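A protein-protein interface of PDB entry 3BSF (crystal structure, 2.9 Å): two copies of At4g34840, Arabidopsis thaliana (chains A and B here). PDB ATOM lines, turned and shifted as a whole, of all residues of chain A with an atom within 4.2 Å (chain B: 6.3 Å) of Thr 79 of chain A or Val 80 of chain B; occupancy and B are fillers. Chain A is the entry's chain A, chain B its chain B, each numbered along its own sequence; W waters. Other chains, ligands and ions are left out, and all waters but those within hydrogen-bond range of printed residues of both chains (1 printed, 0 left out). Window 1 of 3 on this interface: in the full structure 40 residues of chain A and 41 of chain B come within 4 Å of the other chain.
Water W1 lies within hydrogen-bond range of the side-chain carboxylate (OD2) of Asp 166 of chain A, the side-chain carboxylate (OD2) of Asp 166 of chain B, the side-chain hydroxyl (OG1) of Thr 79 of chain B and the side-chain hydroxyl (OG1) of Thr 79 of chain A.
Of the printed residues of chain B, Thr 79 of chain A touches Val 80.
Val 80 of chain B touches just these residues of chain A: Thr 79, Ser 83 and Tyr 195.
Printed residues of chain A within 4 Å of Leu 84 of chain B: Ser 83.
Of the printed residues of chain A, Ser 83 of chain B touches Val 80 (3.9 Å) and Ser 83 (3.8 Å).
Of the printed residues of chain A, Asp 166 of chain B touches Asp 166.
The nearest residue of chain B that does not touch Thr 79 of chain A is Thr 79 of chain B (4.4 Å).
OG of Ser 83 of chain A lies within hydrogen-bond range of O of Thr 79 of chain A, 3.3 Å away.
The side-chain hydroxyl (OG) of Ser 83 of chain A lies within hydrogen-bond range of the backbone carbonyl oxygen (O) of Val 80 of chain A, at 3.1 Å.
The backbone NH (N) of Thr 79 of chain A lies within hydrogen-bond range of the side-chain carboxylate (OD1) of Asp 166 of chain A, at 3.0 Å.
O of Met 188 of chain A lies close to N of Thr 79 of chain A, 3.4 Å away.
The backbone carbonyl oxygen of Val 80 of chain B lies within hydrogen-bond range of the side-chain hydroxyl of Ser 83 of chain B, 3.0 Å away.
The backbone NH (N) of Thr 79 of chain B sits at hydrogen-bond distance from the side-chain carboxylate (OD1) of Asp 166 of chain B, 3.0 Å away.
Of the 12 printed residues of chain A, 5 touch a printed residue of chain B.
Hydrophobic or aromatic side chains of chain A within 4 Å of the printed part of chain B: Val 80 and Tyr 195.
Among the printed residues, no Asp or Glu carboxylate lies within 4 Å of a Lys or Arg side-chain nitrogen of the other chain.
Val 80 of chain B touches Thr 79 of chain A (CG2 to OG1, 3.97 Å).
Val 80 of chain A touches Thr 79 of chain B (CG2 to OG1, 3.96 Å).
Val 80 of chain A touches Ser 83 of chain B.
Val 80 of chain B touches Ser 83 of chain A.
Ser 83 of chain A touches Ser 83 of chain B (OG to OG, 3.8 Å).
CD2 of Leu 84 of chain B touches O of Ser 83 of chain A, 3.9 Å away.
Arg 128 of chain B touches Asp 166 of chain A (CA to O, 3.3 Å).
Asp 166 of chain B touches Asp 166 of chain A.
Val 80 of chain B touches Tyr 195 of chain A.
Thr 79 of chain A touches Val 80 of chain B, and with the chains exchanged Val 80 of chain A touches Thr 79 of chain B.
Val 80 of chain A touches Ser 83 of chain B, and with the chains exchanged Ser 83 of chain A touches Val 80 of chain B.
Ser 83 of chain A touches its own counterpart, Ser 83 of chain B.
Asp 166 of chain B touches its own counterpart, Asp 166 of chain A.
9 positions are printed for both chains.
Of the 9 pairs that touch across the chains among the printed residues, 6 have their exchanged pair printed and touching as well.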
ATOM      1  N   GLY A  78     -27.995  13.248 -22.016  1.00  0.00           N
ATOM      2  CA  GLY A  78     -26.642  13.748 -21.847  1.00  0.00           C
ATOM      3  C   GLY A  78     -25.918  13.971 -23.157  1.00  0.00           C
ATOM      4  O   GLY A  78     -26.343  13.486 -24.201  1.00  0.00           O
ATOM      5  N   THR A  79     -24.808  14.698 -23.095  1.00  0.00           N
ATOM      6  CA  THR A  79     -24.033  15.008 -24.282  1.00  0.00           C
ATOM      7  C   THR A  79     -23.323  13.829 -24.950  1.00  0.00           C
ATOM      8  O   THR A  79     -23.192  13.808 -26.187  1.00  0.00           O
ATOM      9  CB  THR A  79     -22.991  16.117 -24.002  1.00  0.00           C
ATOM     10  OG1 THR A  79     -22.084  15.696 -22.977  1.00  0.00           O
ATOM     11  CG2 THR A  79     -23.687  17.380 -23.582  1.00  0.00           C
ATOM     12  N   VAL A  80     -22.868  12.857 -24.163  1.00  0.00           N
ATOM     13  CA  VAL A  80     -22.186  11.700 -24.749  1.00  0.00           C
ATOM     14  C   VAL A  80     -23.056  10.821 -25.660  1.00  0.00           C
ATOM     15  O   VAL A  80     -22.646  10.493 -26.780  1.00  0.00           O
ATOM     16  CB  VAL A  80     -21.536  10.824 -23.668  1.00  0.00           C
ATOM     17  CG1 VAL A  80     -21.156   9.478 -24.254  1.00  0.00           C
ATOM     18  CG2 VAL A  80     -20.282  11.530 -23.132  1.00  0.00           C
ATOM     19  N   PRO A  81     -24.259  10.424 -25.198  1.00  0.00           N
ATOM     20  CA  PRO A  81     -25.120   9.582 -26.043  1.00  0.00           C
ATOM     21  C   PRO A  81     -25.671  10.387 -27.226  1.00  0.00           C
ATOM     22  O   PRO A  81     -25.875   9.865 -28.316  1.00  0.00           O
ATOM     23  CB  PRO A  81     -26.227   9.144 -25.086  1.00  0.00           C
ATOM     24  CG  PRO A  81     -25.579   9.243 -23.722  1.00  0.00           C
ATOM     25  CD  PRO A  81     -24.805  10.527 -23.836  1.00  0.00           C
ATOM     26  N   ALA A  82     -25.899  11.672 -26.984  1.00  0.00           N
ATOM     27  CA  ALA A  82     -26.424  12.579 -27.992  1.00  0.00           C
ATOM     28  C   ALA A  82     -25.435  12.775 -29.119  1.00  0.00           C
ATOM     29  O   ALA A  82     -25.834  12.935 -30.265  1.00  0.00           O
ATOM     30  CB  ALA A  82     -26.755  13.931 -27.366  1.00  0.00           C
ATOM     31  N   SER A  83     -24.146  12.786 -28.804  1.00  0.00           N
ATOM     32  CA  SER A  83     -23.165  12.974 -29.859  1.00  0.00           C
ATOM     33  C   SER A  83     -22.979  11.662 -30.613  1.00  0.00           C
ATOM     34  O   SER A  83     -23.018  11.651 -31.835  1.00  0.00           O
ATOM     35  CB  SER A  83     -21.823  13.513 -29.306  1.00  0.00           C
ATOM     36  OG  SER A  83     -21.132  12.585 -28.493  1.00  0.00           O
ATOM     37  N   PHE A 125     -21.723  25.527 -24.532  1.00  0.00           N
ATOM     38  CA  PHE A 125     -21.611  24.720 -23.322  1.00  0.00           C
ATOM     39  C   PHE A 125     -21.393  25.643 -22.125  1.00  0.00           C
ATOM     40  O   PHE A 125     -20.590  26.583 -22.193  1.00  0.00           O
ATOM     41  CB  PHE A 125     -20.418  23.751 -23.407  1.00  0.00           C
ATOM     42  CG  PHE A 125     -20.661  22.533 -24.258  1.00  0.00           C
ATOM     43  CD1 PHE A 125     -20.194  22.473 -25.568  1.00  0.00           C
ATOM     44  CD2 PHE A 125     -21.316  21.420 -23.732  1.00  0.00           C
ATOM     45  CE1 PHE A 125     -20.370  21.326 -26.336  1.00  0.00           C
ATOM     46  CE2 PHE A 125     -21.498  20.268 -24.490  1.00  0.00           C
ATOM     47  CZ  PHE A 125     -21.023  20.221 -25.793  1.00  0.00           C
ATOM     48  N   THR A 164     -25.923  24.456 -22.918  1.00  0.00           N
ATOM     49  CA  THR A 164     -26.011  23.021 -22.687  1.00  0.00           C
ATOM     50  C   THR A 164     -25.111  22.554 -21.574  1.00  0.00           C
ATOM     51  O   THR A 164     -24.011  23.070 -21.413  1.00  0.00           O
ATOM     52  CB  THR A 164     -25.681  22.260 -23.977  1.00  0.00           C
ATOM     53  OG1 THR A 164     -26.747  22.456 -24.917  1.00  0.00           O
ATOM     54  CG2 THR A 164     -25.522  20.790 -23.712  1.00  0.00           C
ATOM     55  N   ASP A 166     -24.396  18.858 -18.767  1.00  0.00           N
ATOM     56  CA  ASP A 166     -24.764  17.508 -18.335  1.00  0.00           C
ATOM     57  C   ASP A 166     -25.518  17.398 -17.020  1.00  0.00           C
ATOM     58  O   ASP A 166     -25.833  16.300 -16.572  1.00  0.00           O
ATOM     59  CB  ASP A 166     -23.524  16.600 -18.301  1.00  0.00           C
ATOM     60  CG  ASP A 166     -23.035  16.215 -19.707  1.00  0.00           C
ATOM     61  OD1 ASP A 166     -23.774  15.488 -20.409  1.00  0.00           O
ATOM     62  OD2 ASP A 166     -21.915  16.647 -20.100  1.00  0.00           O
ATOM     63  N   MET A 188     -29.606  19.693 -21.953  1.00  0.00           N
ATOM     64  CA  MET A 188     -28.484  18.781 -21.756  1.00  0.00           C
ATOM     65  C   MET A 188     -27.829  18.138 -22.979  1.00  0.00           C
ATOM     66  O   MET A 188     -26.957  17.280 -22.806  1.00  0.00           O
ATOM     67  CB  MET A 188     -28.909  17.648 -20.825  1.00  0.00           C
ATOM     68  CG  MET A 188     -29.475  18.091 -19.491  1.00  0.00           C
ATOM     69  SD  MET A 188     -29.975  16.654 -18.519  1.00  0.00           S
ATOM     70  CE  MET A 188     -28.357  16.005 -18.012  1.00  0.00           C
ATOM     71  N   ALA A 192     -23.929  19.561 -27.907  1.00  0.00           N
ATOM     72  CA  ALA A 192     -23.222  18.362 -28.368  1.00  0.00           C
ATOM     73  C   ALA A 192     -23.643  17.947 -29.794  1.00  0.00           C
ATOM     74  O   ALA A 192     -22.798  17.596 -30.627  1.00  0.00           O
ATOM     75  CB  ALA A 192     -23.450  17.197 -27.372  1.00  0.00           C
ATOM     76  N   TYR A 195     -22.231  20.161 -32.471  1.00  0.00           N
ATOM     77  CA  TYR A 195     -20.817  19.939 -32.699  1.00  0.00           C
ATOM     78  C   TYR A 195     -20.573  18.881 -33.771  1.00  0.00           C
ATOM     79  O   TYR A 195     -19.828  19.106 -34.725  1.00  0.00           O
ATOM     80  CB  TYR A 195     -20.139  19.487 -31.414  1.00  0.00           C
ATOM     81  CG  TYR A 195     -18.694  19.079 -31.607  1.00  0.00           C
ATOM     82  CD1 TYR A 195     -17.733  20.011 -32.020  1.00  0.00           C
ATOM     83  CD2 TYR A 195     -18.275  17.774 -31.331  1.00  0.00           C
ATOM     84  CE1 TYR A 195     -16.383  19.649 -32.141  1.00  0.00           C
ATOM     85  CE2 TYR A 195     -16.926  17.407 -31.444  1.00  0.00           C
ATOM     86  CZ  TYR A 195     -15.989  18.350 -31.843  1.00  0.00           C
ATOM     87  OH  TYR A 195     -14.659  18.031 -31.877  1.00  0.00           O
ATOM     88  N   VAL B  77     -10.131  18.133 -26.359  1.00  0.00           N
ATOM     89  CA  VAL B  77     -10.279  17.374 -25.111  1.00  0.00           C
ATOM     90  C   VAL B  77     -11.748  17.315 -24.693  1.00  0.00           C
ATOM     91  O   VAL B  77     -12.609  17.942 -25.321  1.00  0.00           O
ATOM     92  CB  VAL B  77      -9.476  18.036 -23.962  1.00  0.00           C
ATOM     93  CG1 VAL B  77      -7.975  18.078 -24.312  1.00  0.00           C
ATOM     94  CG2 VAL B  77     -10.007  19.448 -23.718  1.00  0.00           C
ATOM     95  N   GLY B  78     -12.037  16.564 -23.636  1.00  0.00           N
ATOM     96  CA  GLY B  78     -13.407  16.487 -23.171  1.00  0.00           C
ATOM     97  C   GLY B  78     -14.033  15.154 -23.471  1.00  0.00           C
ATOM     98  O   GLY B  78     -13.495  14.373 -24.256  1.00  0.00           O
ATOM     99  N   THR B  79     -15.187  14.906 -22.858  1.00  0.00           N
ATOM    100  CA  THR B  79     -15.894  13.645 -23.016  1.00  0.00           C
ATOM    101  C   THR B  79     -16.490  13.409 -24.396  1.00  0.00           C
ATOM    102  O   THR B  79     -16.489  12.270 -24.877  1.00  0.00           O
ATOM    103  CB  THR B  79     -17.028  13.482 -21.954  1.00  0.00           C
ATOM    104  OG1 THR B  79     -17.965  14.563 -22.059  1.00  0.00           O
ATOM    105  CG2 THR B  79     -16.439  13.432 -20.566  1.00  0.00           C
ATOM    106  N   VAL B  80     -17.000  14.456 -25.041  1.00  0.00           N
ATOM    107  CA  VAL B  80     -17.603  14.259 -26.358  1.00  0.00           C
ATOM    108  C   VAL B  80     -16.642  13.730 -27.441  1.00  0.00           C
ATOM    109  O   VAL B  80     -16.950  12.744 -28.110  1.00  0.00           O
ATOM    110  CB  VAL B  80     -18.321  15.538 -26.845  1.00  0.00           C
ATOM    111  CG1 VAL B  80     -18.644  15.449 -28.336  1.00  0.00           C
ATOM    112  CG2 VAL B  80     -19.610  15.689 -26.079  1.00  0.00           C
ATOM    113  N   PRO B  81     -15.476  14.379 -27.630  1.00  0.00           N
ATOM    114  CA  PRO B  81     -14.514  13.920 -28.643  1.00  0.00           C
ATOM    115  C   PRO B  81     -13.935  12.559 -28.242  1.00  0.00           C
ATOM    116  O   PRO B  81     -13.657  11.715 -29.096  1.00  0.00           O
ATOM    117  CB  PRO B  81     -13.437  15.010 -28.628  1.00  0.00           C
ATOM    118  CG  PRO B  81     -14.162  16.224 -28.125  1.00  0.00           C
ATOM    119  CD  PRO B  81     -15.028  15.647 -27.029  1.00  0.00           C
ATOM    120  N   ALA B  82     -13.755  12.366 -26.933  1.00  0.00           N
ATOM    121  CA  ALA B  82     -13.204  11.129 -26.384  1.00  0.00           C
ATOM    122  C   ALA B  82     -14.115   9.954 -26.648  1.00  0.00           C
ATOM    123  O   ALA B  82     -13.632   8.843 -26.881  1.00  0.00           O
ATOM    124  CB  ALA B  82     -12.964  11.268 -24.881  1.00  0.00           C
ATOM    125  N   SER B  83     -15.426  10.177 -26.612  1.00  0.00           N
ATOM    126  CA  SER B  83     -16.335   9.069 -26.852  1.00  0.00           C
ATOM    127  C   SER B  83     -16.412   8.777 -28.347  1.00  0.00           C
ATOM    128  O   SER B  83     -16.262   7.627 -28.756  1.00  0.00           O
ATOM    129  CB  SER B  83     -17.729   9.338 -26.241  1.00  0.00           C
ATOM    130  OG  SER B  83     -18.420  10.395 -26.884  1.00  0.00           O
ATOM    131  N   LEU B  84     -16.608   9.813 -29.160  1.00  0.00           N
ATOM    132  CA  LEU B  84     -16.694   9.657 -30.611  1.00  0.00           C
ATOM    133  C   LEU B  84     -15.504   8.832 -31.090  1.00  0.00           C
ATOM    134  O   LEU B  84     -15.671   7.812 -31.755  1.00  0.00           O
ATOM    135  CB  LEU B  84     -16.710  11.029 -31.309  1.00  0.00           C
ATOM    136  CG  LEU B  84     -17.981  11.881 -31.138  1.00  0.00           C
ATOM    137  CD1 LEU B  84     -17.842  13.232 -31.853  1.00  0.00           C
ATOM    138  CD2 LEU B  84     -19.178  11.111 -31.662  1.00  0.00           C
ATOM    139  N   VAL B  85     -14.298   9.276 -30.741  1.00  0.00           N
ATOM    140  CA  VAL B  85     -13.071   8.567 -31.111  1.00  0.00           C
ATOM    141  C   VAL B  85     -13.113   7.097 -30.662  1.00  0.00           C
ATOM    142  O   VAL B  85     -12.848   6.196 -31.446  1.00  0.00           O
ATOM    143  CB  VAL B  85     -11.811   9.266 -30.481  1.00  0.00           C
ATOM    144  CG1 VAL B  85     -10.666   8.275 -30.311  1.00  0.00           C
ATOM    145  CG2 VAL B  85     -11.365  10.429 -31.367  1.00  0.00           C
ATOM    146  N   ARG B 128     -22.290  15.298 -13.836  1.00  0.00           N
ATOM    147  CA  ARG B 128     -23.570  14.986 -14.504  1.00  0.00           C
ATOM    148  C   ARG B 128     -24.643  14.749 -13.442  1.00  0.00           C
ATOM    149  O   ARG B 128     -25.203  13.658 -13.315  1.00  0.00           O
ATOM    150  CB  ARG B 128     -23.455  13.734 -15.399  1.00  0.00           C
ATOM    151  CG  ARG B 128     -22.334  13.792 -16.428  1.00  0.00           C
ATOM    152  CD  ARG B 128     -22.590  12.856 -17.602  1.00  0.00           C
ATOM    153  NE  ARG B 128     -22.883  11.482 -17.192  1.00  0.00           N
ATOM    154  CZ  ARG B 128     -23.260  10.517 -18.029  1.00  0.00           C
ATOM    155  NH1 ARG B 128     -23.390  10.768 -19.323  1.00  0.00           N
ATOM    156  NH2 ARG B 128     -23.520   9.299 -17.568  1.00  0.00           N
ATOM    157  N   ASP B 166     -16.040  17.533 -17.483  1.00  0.00           N
ATOM    158  CA  ASP B 166     -15.642  18.406 -18.584  1.00  0.00           C
ATOM    159  C   ASP B 166     -14.965  19.718 -18.184  1.00  0.00           C
ATOM    160  O   ASP B 166     -14.630  20.535 -19.034  1.00  0.00           O
ATOM    161  CB  ASP B 166     -16.855  18.694 -19.480  1.00  0.00           C
ATOM    162  CG  ASP B 166     -17.247  17.498 -20.321  1.00  0.00           C
ATOM    163  OD1 ASP B 166     -16.427  17.101 -21.176  1.00  0.00           O
ATOM    164  OD2 ASP B 166     -18.364  16.958 -20.121  1.00  0.00           O
ATOM    165  N   MET B 188     -10.686  14.511 -17.476  1.00  0.00           N
ATOM    166  CA  MET B 188     -11.770  14.952 -18.348  1.00  0.00           C
ATOM    167  C   MET B 188     -12.319  13.983 -19.398  1.00  0.00           C
ATOM    168  O   MET B 188     -13.182  14.368 -20.191  1.00  0.00           O
ATOM    169  CB  MET B 188     -11.339  16.225 -19.067  1.00  0.00           C
ATOM    170  CG  MET B 188     -10.915  17.364 -18.155  1.00  0.00           C
ATOM    171  SD  MET B 188     -10.394  18.829 -19.110  1.00  0.00           S
ATOM    172  CE  MET B 188     -12.007  19.440 -19.689  1.00  0.00           C
ATOM    173  N   ALA B 192     -15.954   8.637 -19.930  1.00  0.00           N
ATOM    174  CA  ALA B 192     -16.592   8.618 -21.246  1.00  0.00           C
ATOM    175  C   ALA B 192     -16.071   7.458 -22.095  1.00  0.00           C
ATOM    176  O   ALA B 192     -16.851   6.771 -22.769  1.00  0.00           O
ATOM    177  CB  ALA B 192     -16.357   9.960 -21.967  1.00  0.00           C
HETATM  178  O   HOH W   1     -20.052  14.837 -20.287  1.00  0.00           O
